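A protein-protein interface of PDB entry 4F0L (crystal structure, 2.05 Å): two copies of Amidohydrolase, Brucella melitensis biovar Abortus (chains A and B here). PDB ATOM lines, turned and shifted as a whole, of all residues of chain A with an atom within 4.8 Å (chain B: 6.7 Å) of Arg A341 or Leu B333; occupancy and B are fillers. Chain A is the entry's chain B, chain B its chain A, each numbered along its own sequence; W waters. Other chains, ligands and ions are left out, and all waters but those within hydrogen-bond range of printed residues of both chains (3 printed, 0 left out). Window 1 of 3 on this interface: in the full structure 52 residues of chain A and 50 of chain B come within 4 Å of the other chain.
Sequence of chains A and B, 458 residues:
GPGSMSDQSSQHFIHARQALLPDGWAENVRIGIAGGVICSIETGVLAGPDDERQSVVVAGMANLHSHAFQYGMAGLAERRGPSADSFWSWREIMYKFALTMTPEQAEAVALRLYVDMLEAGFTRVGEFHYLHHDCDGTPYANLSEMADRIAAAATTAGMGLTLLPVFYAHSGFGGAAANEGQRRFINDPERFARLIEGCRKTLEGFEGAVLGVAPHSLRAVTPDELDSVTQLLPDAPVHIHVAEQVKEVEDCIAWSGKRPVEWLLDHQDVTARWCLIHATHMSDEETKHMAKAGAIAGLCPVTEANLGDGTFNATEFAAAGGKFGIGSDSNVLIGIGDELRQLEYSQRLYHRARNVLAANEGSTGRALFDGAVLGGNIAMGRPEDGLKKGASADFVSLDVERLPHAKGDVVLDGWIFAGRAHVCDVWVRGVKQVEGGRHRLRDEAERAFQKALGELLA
N of Val B332 sits close to OG of Ser B330, at 3.5 Å. The backbone carbonyl oxygen of Gly A337 sits close to the guanidinium group of Arg A341, 3.4 Å away. The guanidinium group (NH1) of Arg A341 lies within salt-bridge range of the side-chain carboxylate (OD1) of Asp A338, 3.1 Å away. The backbone carbonyl oxygen of Ile A416 is in hydrogen-bond range of the guanidinium group of Arg A341 (2.9 Å).
O of Ala A418 sits close to O of Val B332, 3.4 Å away.
Hydrophobic or aromatic side chains of chain A within 4 Å of the printed part of chain B: Ala A418. Along chain A the printed residues that touch a printed residue of chain B span positions 341 to 419. Among the printed residues, no Asp or Glu carboxylate lies within 4 Å of a Lys or Arg side-chain nitrogen of the other chain.
Arg A341 touches Leu B333. Phe A417 touches Val B332 (O to CG2, 3.8 Å). Leu B333 touches Phe A417 (CB to O, 3.7 Å). Ala B74 touches Ala A418. CD1 of Leu B333 touches O of Ala A418, at 3.5 Å. Leu B333 touches Gly A419.
Water W3 lies within hydrogen-bond range of OD1 of Asp B338 (2.6 Å), NH1 of Arg A341 (2.8 Å) and NH1 of Arg B341 (3.4 Å). Water W1 bridges the side-chain carboxylate (OD1) of Asp A338 (2.7 Å) and the guanidinium group (NH1) of Arg B341 (2.9 Å). Water W2 bridges N of Ile B334 (3.0 Å) and O of Ala A418 (3.2 Å).
Of chain B, only Leu B333 (3.8 Å) comes within 4 Å of Arg A341. Of the printed residues of chain B, Phe A417 touches Val B332 (3.8 Å) and Leu B333 (3.7 Å). Printed residues of chain B within 4 Å of Ala A418: Ala B74 (3.8 Å), Val B332 (3.1 Å) and Leu B333 (3.5 Å). Printed residues of chain B within 4 Å of Gly A419: Leu B333. Of the printed residues of chain A, Ala B74 touches Ala A418. Of the printed residues of chain A, Val B332 touches Phe A417 (3.8 Å) and Ala A418 (3.1 Å). Of chain A, only Arg A341 (3.8 Å), Phe A417 (3.7 Å), Ala A418 (3.5 Å) and Gly A419 (3.7 Å) come within 4 Å of Leu B333. The nearest residue of chain B that does not touch Arg A341 is Asp B338 (4.1 Å). The nearest printed residue of chain A that does not touch Leu B333 is Ile A416 (5.3 Å). The nearest printed residue of chain B that does not touch Phe A417 is Val B302 (6.0 Å).
Positions printed for both chains: 338, 339 and 341. Of the 7 pairs that touch across the chains among the printed residues, none has its exchanged pair printed and touching as well.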
ATOM      1  N   ILE A 336      18.783   8.517 -20.493  1.00  0.00           N
ATOM      2  CA  ILE A 336      17.310   8.622 -20.555  1.00  0.00           C
ATOM      3  C   ILE A 336      16.800   8.774 -19.138  1.00  0.00           C
ATOM      4  O   ILE A 336      15.955   9.609 -18.883  1.00  0.00           O
ATOM      5  CB  ILE A 336      16.675   7.381 -21.232  1.00  0.00           C
ATOM      6  CG1 ILE A 336      17.032   7.328 -22.731  1.00  0.00           C
ATOM      7  CG2 ILE A 336      15.182   7.343 -20.959  1.00  0.00           C
ATOM      8  CD1 ILE A 336      16.560   6.097 -23.488  1.00  0.00           C
ATOM      9  N   GLY A 337      17.292   7.954 -18.228  1.00  0.00           N
ATOM     10  CA  GLY A 337      16.903   8.065 -16.813  1.00  0.00           C
ATOM     11  C   GLY A 337      17.226   9.443 -16.242  1.00  0.00           C
ATOM     12  O   GLY A 337      16.415  10.076 -15.559  1.00  0.00           O
ATOM     13  N   ASP A 338      18.404   9.943 -16.572  1.00  0.00           N
ATOM     14  CA  ASP A 338      18.822  11.242 -16.101  1.00  0.00           C
ATOM     15  C   ASP A 338      17.877  12.361 -16.524  1.00  0.00           C
ATOM     16  O   ASP A 338      17.514  13.189 -15.696  1.00  0.00           O
ATOM     17  CB  ASP A 338      20.244  11.519 -16.557  1.00  0.00           C
ATOM     18  CG  ASP A 338      21.208  10.481 -16.032  1.00  0.00           C
ATOM     19  OD1 ASP A 338      21.635  10.566 -14.872  1.00  0.00           O
ATOM     20  OD2 ASP A 338      21.488   9.546 -16.764  1.00  0.00           O
ATOM     21  N   GLU A 339      17.496  12.376 -17.802  1.00  0.00           N
ATOM     22  CA  GLU A 339      16.611  13.389 -18.299  1.00  0.00           C
ATOM     23  C   GLU A 339      15.188  13.301 -17.745  1.00  0.00           C
ATOM     24  O   GLU A 339      14.596  14.310 -17.305  1.00  0.00           O
ATOM     25  CB  GLU A 339      16.558  13.381 -19.823  1.00  0.00           C
ATOM     26  CG  GLU A 339      17.891  13.673 -20.475  1.00  0.00           C
ATOM     27  CD  GLU A 339      18.362  15.121 -20.394  1.00  0.00           C
ATOM     28  OE1 GLU A 339      17.623  15.956 -19.869  1.00  0.00           O
ATOM     29  OE2 GLU A 339      19.504  15.416 -20.848  1.00  0.00           O
ATOM     30  N   LEU A 340      14.626  12.104 -17.762  1.00  0.00           N
ATOM     31  CA  LEU A 340      13.249  11.928 -17.331  1.00  0.00           C
ATOM     32  C   LEU A 340      13.147  12.166 -15.831  1.00  0.00           C
ATOM     33  O   LEU A 340      12.167  12.795 -15.344  1.00  0.00           O
ATOM     34  CB  LEU A 340      12.731  10.538 -17.704  1.00  0.00           C
ATOM     35  CG  LEU A 340      12.582  10.288 -19.208  1.00  0.00           C
ATOM     36  CD1 LEU A 340      12.012   8.888 -19.469  1.00  0.00           C
ATOM     37  CD2 LEU A 340      11.731  11.387 -19.866  1.00  0.00           C
ATOM     38  N   ARG A 341      14.101  11.629 -15.078  1.00  0.00           N
ATOM     39  CA  ARG A 341      14.111  11.847 -13.639  1.00  0.00           C
ATOM     40  C   ARG A 341      14.166  13.343 -13.344  1.00  0.00           C
ATOM     41  O   ARG A 341      13.408  13.850 -12.498  1.00  0.00           O
ATOM     42  CB  ARG A 341      15.302  11.115 -13.033  1.00  0.00           C
ATOM     43  CG  ARG A 341      15.387  11.129 -11.566  1.00  0.00           C
ATOM     44  CD  ARG A 341      16.361  10.052 -11.061  1.00  0.00           C
ATOM     45  NE  ARG A 341      17.730  10.327 -11.451  1.00  0.00           N
ATOM     46  CZ  ARG A 341      18.462   9.617 -12.317  1.00  0.00           C
ATOM     47  NH1 ARG A 341      19.702  10.001 -12.579  1.00  0.00           N
ATOM     48  NH2 ARG A 341      18.009   8.534 -12.927  1.00  0.00           N
ATOM     49  N   GLN A 342      15.079  14.052 -14.002  1.00  0.00           N
ATOM     50  CA  GLN A 342      15.201  15.507 -13.790  1.00  0.00           C
ATOM     51  C   GLN A 342      13.905  16.259 -14.145  1.00  0.00           C
ATOM     52  O   GLN A 342      13.478  17.153 -13.407  1.00  0.00           O
ATOM     53  CB  GLN A 342      16.401  16.067 -14.540  1.00  0.00           C
ATOM     54  CG  GLN A 342      16.571  17.594 -14.488  1.00  0.00           C
ATOM     55  CD  GLN A 342      16.755  18.124 -13.089  1.00  0.00           C
ATOM     56  OE1 GLN A 342      17.389  17.471 -12.270  1.00  0.00           O
ATOM     57  NE2 GLN A 342      16.161  19.292 -12.784  1.00  0.00           N
ATOM     58  N   LEU A 343      13.258  15.870 -15.247  1.00  0.00           N
ATOM     59  CA  LEU A 343      11.971  16.454 -15.583  1.00  0.00           C
ATOM     60  C   LEU A 343      10.960  16.287 -14.429  1.00  0.00           C
ATOM     61  O   LEU A 343      10.422  17.283 -13.917  1.00  0.00           O
ATOM     62  CB  LEU A 343      11.435  15.851 -16.873  1.00  0.00           C
ATOM     63  CG  LEU A 343      10.053  16.291 -17.331  1.00  0.00           C
ATOM     64  CD1 LEU A 343       9.955  17.810 -17.493  1.00  0.00           C
ATOM     65  CD2 LEU A 343       9.684  15.515 -18.611  1.00  0.00           C
ATOM     66  N   GLU A 344      10.754  15.054 -13.976  1.00  0.00           N
ATOM     67  CA  GLU A 344       9.814  14.801 -12.911  1.00  0.00           C
ATOM     68  C   GLU A 344      10.204  15.529 -11.643  1.00  0.00           C
ATOM     69  O   GLU A 344       9.346  16.157 -11.004  1.00  0.00           O
ATOM     70  CB  GLU A 344       9.689  13.286 -12.674  1.00  0.00           C
ATOM     71  CG  GLU A 344       8.860  12.827 -11.457  1.00  0.00           C
ATOM     72  CD  GLU A 344       7.390  13.199 -11.488  1.00  0.00           C
ATOM     73  OE1 GLU A 344       6.828  13.592 -12.560  1.00  0.00           O
ATOM     74  OE2 GLU A 344       6.770  13.105 -10.404  1.00  0.00           O
ATOM     75  N   TYR A 345      11.478  15.433 -11.259  1.00  0.00           N
ATOM     76  CA  TYR A 345      11.891  15.970  -9.984  1.00  0.00           C
ATOM     77  C   TYR A 345      11.795  17.491  -9.992  1.00  0.00           C
ATOM     78  O   TYR A 345      11.512  18.085  -8.956  1.00  0.00           O
ATOM     79  CB  TYR A 345      13.299  15.511  -9.555  1.00  0.00           C
ATOM     80  CG  TYR A 345      13.414  14.052  -9.079  1.00  0.00           C
ATOM     81  CD1 TYR A 345      12.298  13.226  -8.941  1.00  0.00           C
ATOM     82  CD2 TYR A 345      14.634  13.541  -8.710  1.00  0.00           C
ATOM     83  CE1 TYR A 345      12.411  11.913  -8.481  1.00  0.00           C
ATOM     84  CE2 TYR A 345      14.763  12.227  -8.263  1.00  0.00           C
ATOM     85  CZ  TYR A 345      13.643  11.429  -8.109  1.00  0.00           C
ATOM     86  OH  TYR A 345      13.796  10.142  -7.644  1.00  0.00           O
ATOM     87  N   SER A 346      12.008  18.131 -11.144  1.00  0.00           N
ATOM     88  CA  SER A 346      11.865  19.574 -11.222  1.00  0.00           C
ATOM     89  C   SER A 346      10.411  19.886 -10.868  1.00  0.00           C
ATOM     90  O   SER A 346      10.130  20.890 -10.188  1.00  0.00           O
ATOM     91  CB  SER A 346      12.260  20.132 -12.597  1.00  0.00           C
ATOM     92  OG  SER A 346      11.384  19.730 -13.642  1.00  0.00           O
ATOM     93  N   ILE A 416      14.391   4.228 -14.140  1.00  0.00           N
ATOM     94  CA  ILE A 416      14.461   5.688 -14.208  1.00  0.00           C
ATOM     95  C   ILE A 416      14.722   6.331 -12.849  1.00  0.00           C
ATOM     96  O   ILE A 416      15.430   7.318 -12.777  1.00  0.00           O
ATOM     97  CB  ILE A 416      13.164   6.261 -14.803  1.00  0.00           C
ATOM     98  CG1 ILE A 416      13.082   5.901 -16.286  1.00  0.00           C
ATOM     99  CG2 ILE A 416      13.085   7.783 -14.594  1.00  0.00           C
ATOM    100  CD1 ILE A 416      11.684   6.026 -16.878  1.00  0.00           C
ATOM    101  N   PHE A 417      14.162   5.781 -11.774  1.00  0.00           N
ATOM    102  CA  PHE A 417      14.241   6.422 -10.460  1.00  0.00           C
ATOM    103  C   PHE A 417      15.185   5.799  -9.469  1.00  0.00           C
ATOM    104  O   PHE A 417      15.650   6.464  -8.578  1.00  0.00           O
ATOM    105  CB  PHE A 417      12.840   6.542  -9.846  1.00  0.00           C
ATOM    106  CG  PHE A 417      11.931   7.449 -10.626  1.00  0.00           C
ATOM    107  CD1 PHE A 417      12.091   8.825 -10.575  1.00  0.00           C
ATOM    108  CD2 PHE A 417      10.959   6.926 -11.471  1.00  0.00           C
ATOM    109  CE1 PHE A 417      11.268   9.670 -11.300  1.00  0.00           C
ATOM    110  CE2 PHE A 417      10.144   7.772 -12.219  1.00  0.00           C
ATOM    111  CZ  PHE A 417      10.290   9.144 -12.133  1.00  0.00           C
ATOM    112  N   ALA A 418      15.427   4.501  -9.589  1.00  0.00           N
ATOM    113  CA  ALA A 418      16.152   3.769  -8.551  1.00  0.00           C
ATOM    114  C   ALA A 418      17.471   3.210  -9.032  1.00  0.00           C
ATOM    115  O   ALA A 418      18.165   2.616  -8.241  1.00  0.00           O
ATOM    116  CB  ALA A 418      15.293   2.654  -7.970  1.00  0.00           C
ATOM    117  N   GLY A 419      17.805   3.368 -10.314  1.00  0.00           N
ATOM    118  CA  GLY A 419      19.085   2.860 -10.833  1.00  0.00           C
ATOM    119  C   GLY A 419      19.164   1.334 -10.819  1.00  0.00           C
ATOM    120  O   GLY A 419      20.258   0.755 -10.792  1.00  0.00           O
ATOM    121  N   TYR B  71      15.519   1.024   1.445  1.00  0.00           N
ATOM    122  CA  TYR B  71      16.205   0.525   0.242  1.00  0.00           C
ATOM    123  C   TYR B  71      15.378  -0.559  -0.446  1.00  0.00           C
ATOM    124  O   TYR B  71      15.398  -0.663  -1.653  1.00  0.00           O
ATOM    125  CB  TYR B  71      17.563  -0.060   0.612  1.00  0.00           C
ATOM    126  CG  TYR B  71      18.462  -0.582  -0.537  1.00  0.00           C
ATOM    127  CD1 TYR B  71      19.091   0.293  -1.439  1.00  0.00           C
ATOM    128  CD2 TYR B  71      18.716  -1.923  -0.662  1.00  0.00           C
ATOM    129  CE1 TYR B  71      19.942  -0.174  -2.432  1.00  0.00           C
ATOM    130  CE2 TYR B  71      19.580  -2.412  -1.626  1.00  0.00           C
ATOM    131  CZ  TYR B  71      20.184  -1.536  -2.523  1.00  0.00           C
ATOM    132  OH  TYR B  71      21.029  -2.049  -3.474  1.00  0.00           O
ATOM    133  N   ALA B  74      12.846   0.971  -2.914  1.00  0.00           N
ATOM    134  CA  ALA B  74      13.371   1.852  -3.969  1.00  0.00           C
ATOM    135  C   ALA B  74      12.775   1.479  -5.335  1.00  0.00           C
ATOM    136  O   ALA B  74      12.792   0.304  -5.743  1.00  0.00           O
ATOM    137  CB  ALA B  74      14.900   1.770  -4.038  1.00  0.00           C
ATOM    138  N   VAL B 302      18.688  13.940  -3.169  1.00  0.00           N
ATOM    139  CA  VAL B 302      17.914  13.050  -4.011  1.00  0.00           C
ATOM    140  C   VAL B 302      16.572  12.704  -3.374  1.00  0.00           C
ATOM    141  O   VAL B 302      15.544  12.745  -4.043  1.00  0.00           O
ATOM    142  CB  VAL B 302      18.705  11.772  -4.380  1.00  0.00           C
ATOM    143  CG1 VAL B 302      17.798  10.732  -5.032  1.00  0.00           C
ATOM    144  CG2 VAL B 302      19.889  12.148  -5.301  1.00  0.00           C
ATOM    145  N   THR B 303      16.571  12.364  -2.092  1.00  0.00           N
ATOM    146  CA  THR B 303      15.337  12.026  -1.419  1.00  0.00           C
ATOM    147  C   THR B 303      14.429  13.243  -1.344  1.00  0.00           C
ATOM    148  O   THR B 303      13.217  13.132  -1.544  1.00  0.00           O
ATOM    149  CB  THR B 303      15.578  11.425  -0.026  1.00  0.00           C
ATOM    150  OG1 THR B 303      16.285  10.178  -0.175  1.00  0.00           O
ATOM    151  CG2 THR B 303      14.225  11.198   0.675  1.00  0.00           C
ATOM    152  N   SER B 328      21.755   9.393   1.795  1.00  0.00           N
ATOM    153  CA  SER B 328      20.852   8.764   0.837  1.00  0.00           C
ATOM    154  C   SER B 328      19.400   8.624   1.358  1.00  0.00           C
ATOM    155  O   SER B 328      18.485   8.493   0.558  1.00  0.00           O
ATOM    156  CB  SER B 328      21.393   7.380   0.455  1.00  0.00           C
ATOM    157  OG  SER B 328      22.624   7.527  -0.221  1.00  0.00           O
ATOM    158  N   SER B 330      16.106   7.937   2.020  1.00  0.00           N
ATOM    159  CA  SER B 330      15.157   6.914   1.572  1.00  0.00           C
ATOM    160  C   SER B 330      15.837   5.778   0.846  1.00  0.00           C
ATOM    161  O   SER B 330      15.242   4.719   0.615  1.00  0.00           O
ATOM    162  CB  SER B 330      14.048   7.517   0.671  1.00  0.00           C
ATOM    163  OG  SER B 330      14.565   7.889  -0.614  1.00  0.00           O
ATOM    164  N   ASN B 331      17.060   6.045   0.406  1.00  0.00           N
ATOM    165  CA  ASN B 331      17.894   5.037  -0.275  1.00  0.00           C
ATOM    166  C   ASN B 331      17.288   4.623  -1.623  1.00  0.00           C
ATOM    167  O   ASN B 331      17.524   3.517  -2.114  1.00  0.00           O
ATOM    168  CB  ASN B 331      18.165   3.839   0.649  1.00  0.00           C
ATOM    169  CG  ASN B 331      19.060   4.216   1.822  1.00  0.00           C
ATOM    170  OD1 ASN B 331      20.059   4.894   1.632  1.00  0.00           O
ATOM    171  ND2 ASN B 331      18.722   3.765   3.040  1.00  0.00           N
ATOM    172  N   VAL B 332      16.548   5.538  -2.231  1.00  0.00           N
ATOM    173  CA  VAL B 332      15.921   5.271  -3.521  1.00  0.00           C
ATOM    174  C   VAL B 332      16.964   5.163  -4.652  1.00  0.00           C
ATOM    175  O   VAL B 332      16.831   4.327  -5.581  1.00  0.00           O
ATOM    176  CB  VAL B 332      14.822   6.342  -3.870  1.00  0.00           C
ATOM    177  CG1 VAL B 332      15.426   7.743  -4.015  1.00  0.00           C
ATOM    178  CG2 VAL B 332      14.069   5.916  -5.134  1.00  0.00           C
ATOM    179  N   LEU B 333      18.015   5.973  -4.560  1.00  0.00           N
ATOM    180  CA  LEU B 333      19.104   5.954  -5.540  1.00  0.00           C
ATOM    181  C   LEU B 333      20.388   6.338  -4.835  1.00  0.00           C
ATOM    182  O   LEU B 333      20.428   7.380  -4.176  1.00  0.00           O
ATOM    183  CB  LEU B 333      18.805   6.946  -6.694  1.00  0.00           C
ATOM    184  CG  LEU B 333      19.775   7.001  -7.877  1.00  0.00           C
ATOM    185  CD1 LEU B 333      19.995   5.586  -8.381  1.00  0.00           C
ATOM    186  CD2 LEU B 333      19.207   7.816  -9.044  1.00  0.00           C
ATOM    187  N   ILE B 334      21.436   5.510  -5.000  1.00  0.00           N
ATOM    188  CA  ILE B 334      22.638   5.619  -4.222  1.00  0.00           C
ATOM    189  C   ILE B 334      23.773   6.190  -5.086  1.00  0.00           C
ATOM    190  O   ILE B 334      24.178   5.552  -6.035  1.00  0.00           O
ATOM    191  CB  ILE B 334      23.115   4.254  -3.671  1.00  0.00           C
ATOM    192  CG1 ILE B 334      22.025   3.522  -2.899  1.00  0.00           C
ATOM    193  CG2 ILE B 334      24.322   4.475  -2.756  1.00  0.00           C
ATOM    194  CD1 ILE B 334      21.410   4.300  -1.719  1.00  0.00           C
ATOM    195  N   GLY B 335      24.279   7.378  -4.759  1.00  0.00           N
ATOM    196  CA  GLY B 335      25.392   7.941  -5.520  1.00  0.00           C
ATOM    197  C   GLY B 335      25.878   9.274  -4.962  1.00  0.00           C
ATOM    198  O   GLY B 335      25.070  10.137  -4.641  1.00  0.00           O
ATOM    199  N   ASP B 338      25.188  11.753  -7.773  1.00  0.00           N
ATOM    200  CA  ASP B 338      23.755  12.016  -7.810  1.00  0.00           C
ATOM    201  C   ASP B 338      23.331  13.017  -6.776  1.00  0.00           C
ATOM    202  O   ASP B 338      22.580  13.939  -7.084  1.00  0.00           O
ATOM    203  CB  ASP B 338      22.978  10.706  -7.647  1.00  0.00           C
ATOM    204  CG  ASP B 338      23.294   9.753  -8.747  1.00  0.00           C
ATOM    205  OD1 ASP B 338      22.721   9.878  -9.841  1.00  0.00           O
ATOM    206  OD2 ASP B 338      24.207   8.946  -8.560  1.00  0.00           O
ATOM    207  N   GLU B 339      23.818  12.854  -5.534  1.00  0.00           N
ATOM    208  CA  GLU B 339      23.444  13.771  -4.462  1.00  0.00           C
ATOM    209  C   GLU B 339      24.040  15.194  -4.650  1.00  0.00           C
ATOM    210  O   GLU B 339      23.329  16.207  -4.472  1.00  0.00           O
ATOM    211  CB  GLU B 339      23.854  13.228  -3.087  1.00  0.00           C
ATOM    212  CG  GLU B 339      23.187  11.898  -2.710  1.00  0.00           C
ATOM    213  CD  GLU B 339      21.714  12.000  -2.353  1.00  0.00           C
ATOM    214  OE1 GLU B 339      21.198  13.142  -2.308  1.00  0.00           O
ATOM    215  OE2 GLU B 339      21.076  10.920  -2.110  1.00  0.00           O
ATOM    216  N   ARG B 341      25.312  16.621  -7.377  1.00  0.00           N
ATOM    217  CA  ARG B 341      24.727  17.232  -8.555  1.00  0.00           C
ATOM    218  C   ARG B 341      23.327  17.783  -8.269  1.00  0.00           C
ATOM    219  O   ARG B 341      22.993  18.924  -8.636  1.00  0.00           O
ATOM    220  CB  ARG B 341      24.653  16.206  -9.656  1.00  0.00           C
ATOM    221  CG  ARG B 341      24.204  16.699 -10.994  1.00  0.00           C
ATOM    222  CD  ARG B 341      24.593  15.696 -12.095  1.00  0.00           C
ATOM    223  NE  ARG B 341      23.850  14.455 -11.953  1.00  0.00           N
ATOM    224  CZ  ARG B 341      24.338  13.266 -11.647  1.00  0.00           C
ATOM    225  NH1 ARG B 341      23.507  12.240 -11.577  1.00  0.00           N
ATOM    226  NH2 ARG B 341      25.622  13.055 -11.417  1.00  0.00           N
HETATM  227  O   HOH W   1      21.429  12.891 -13.536  1.00  0.00           O
HETATM  228  O   HOH W   2      21.044   3.297  -6.924  1.00  0.00           O
HETATM  229  O   HOH W   3      20.533  11.166 -10.220  1.00  0.00           O
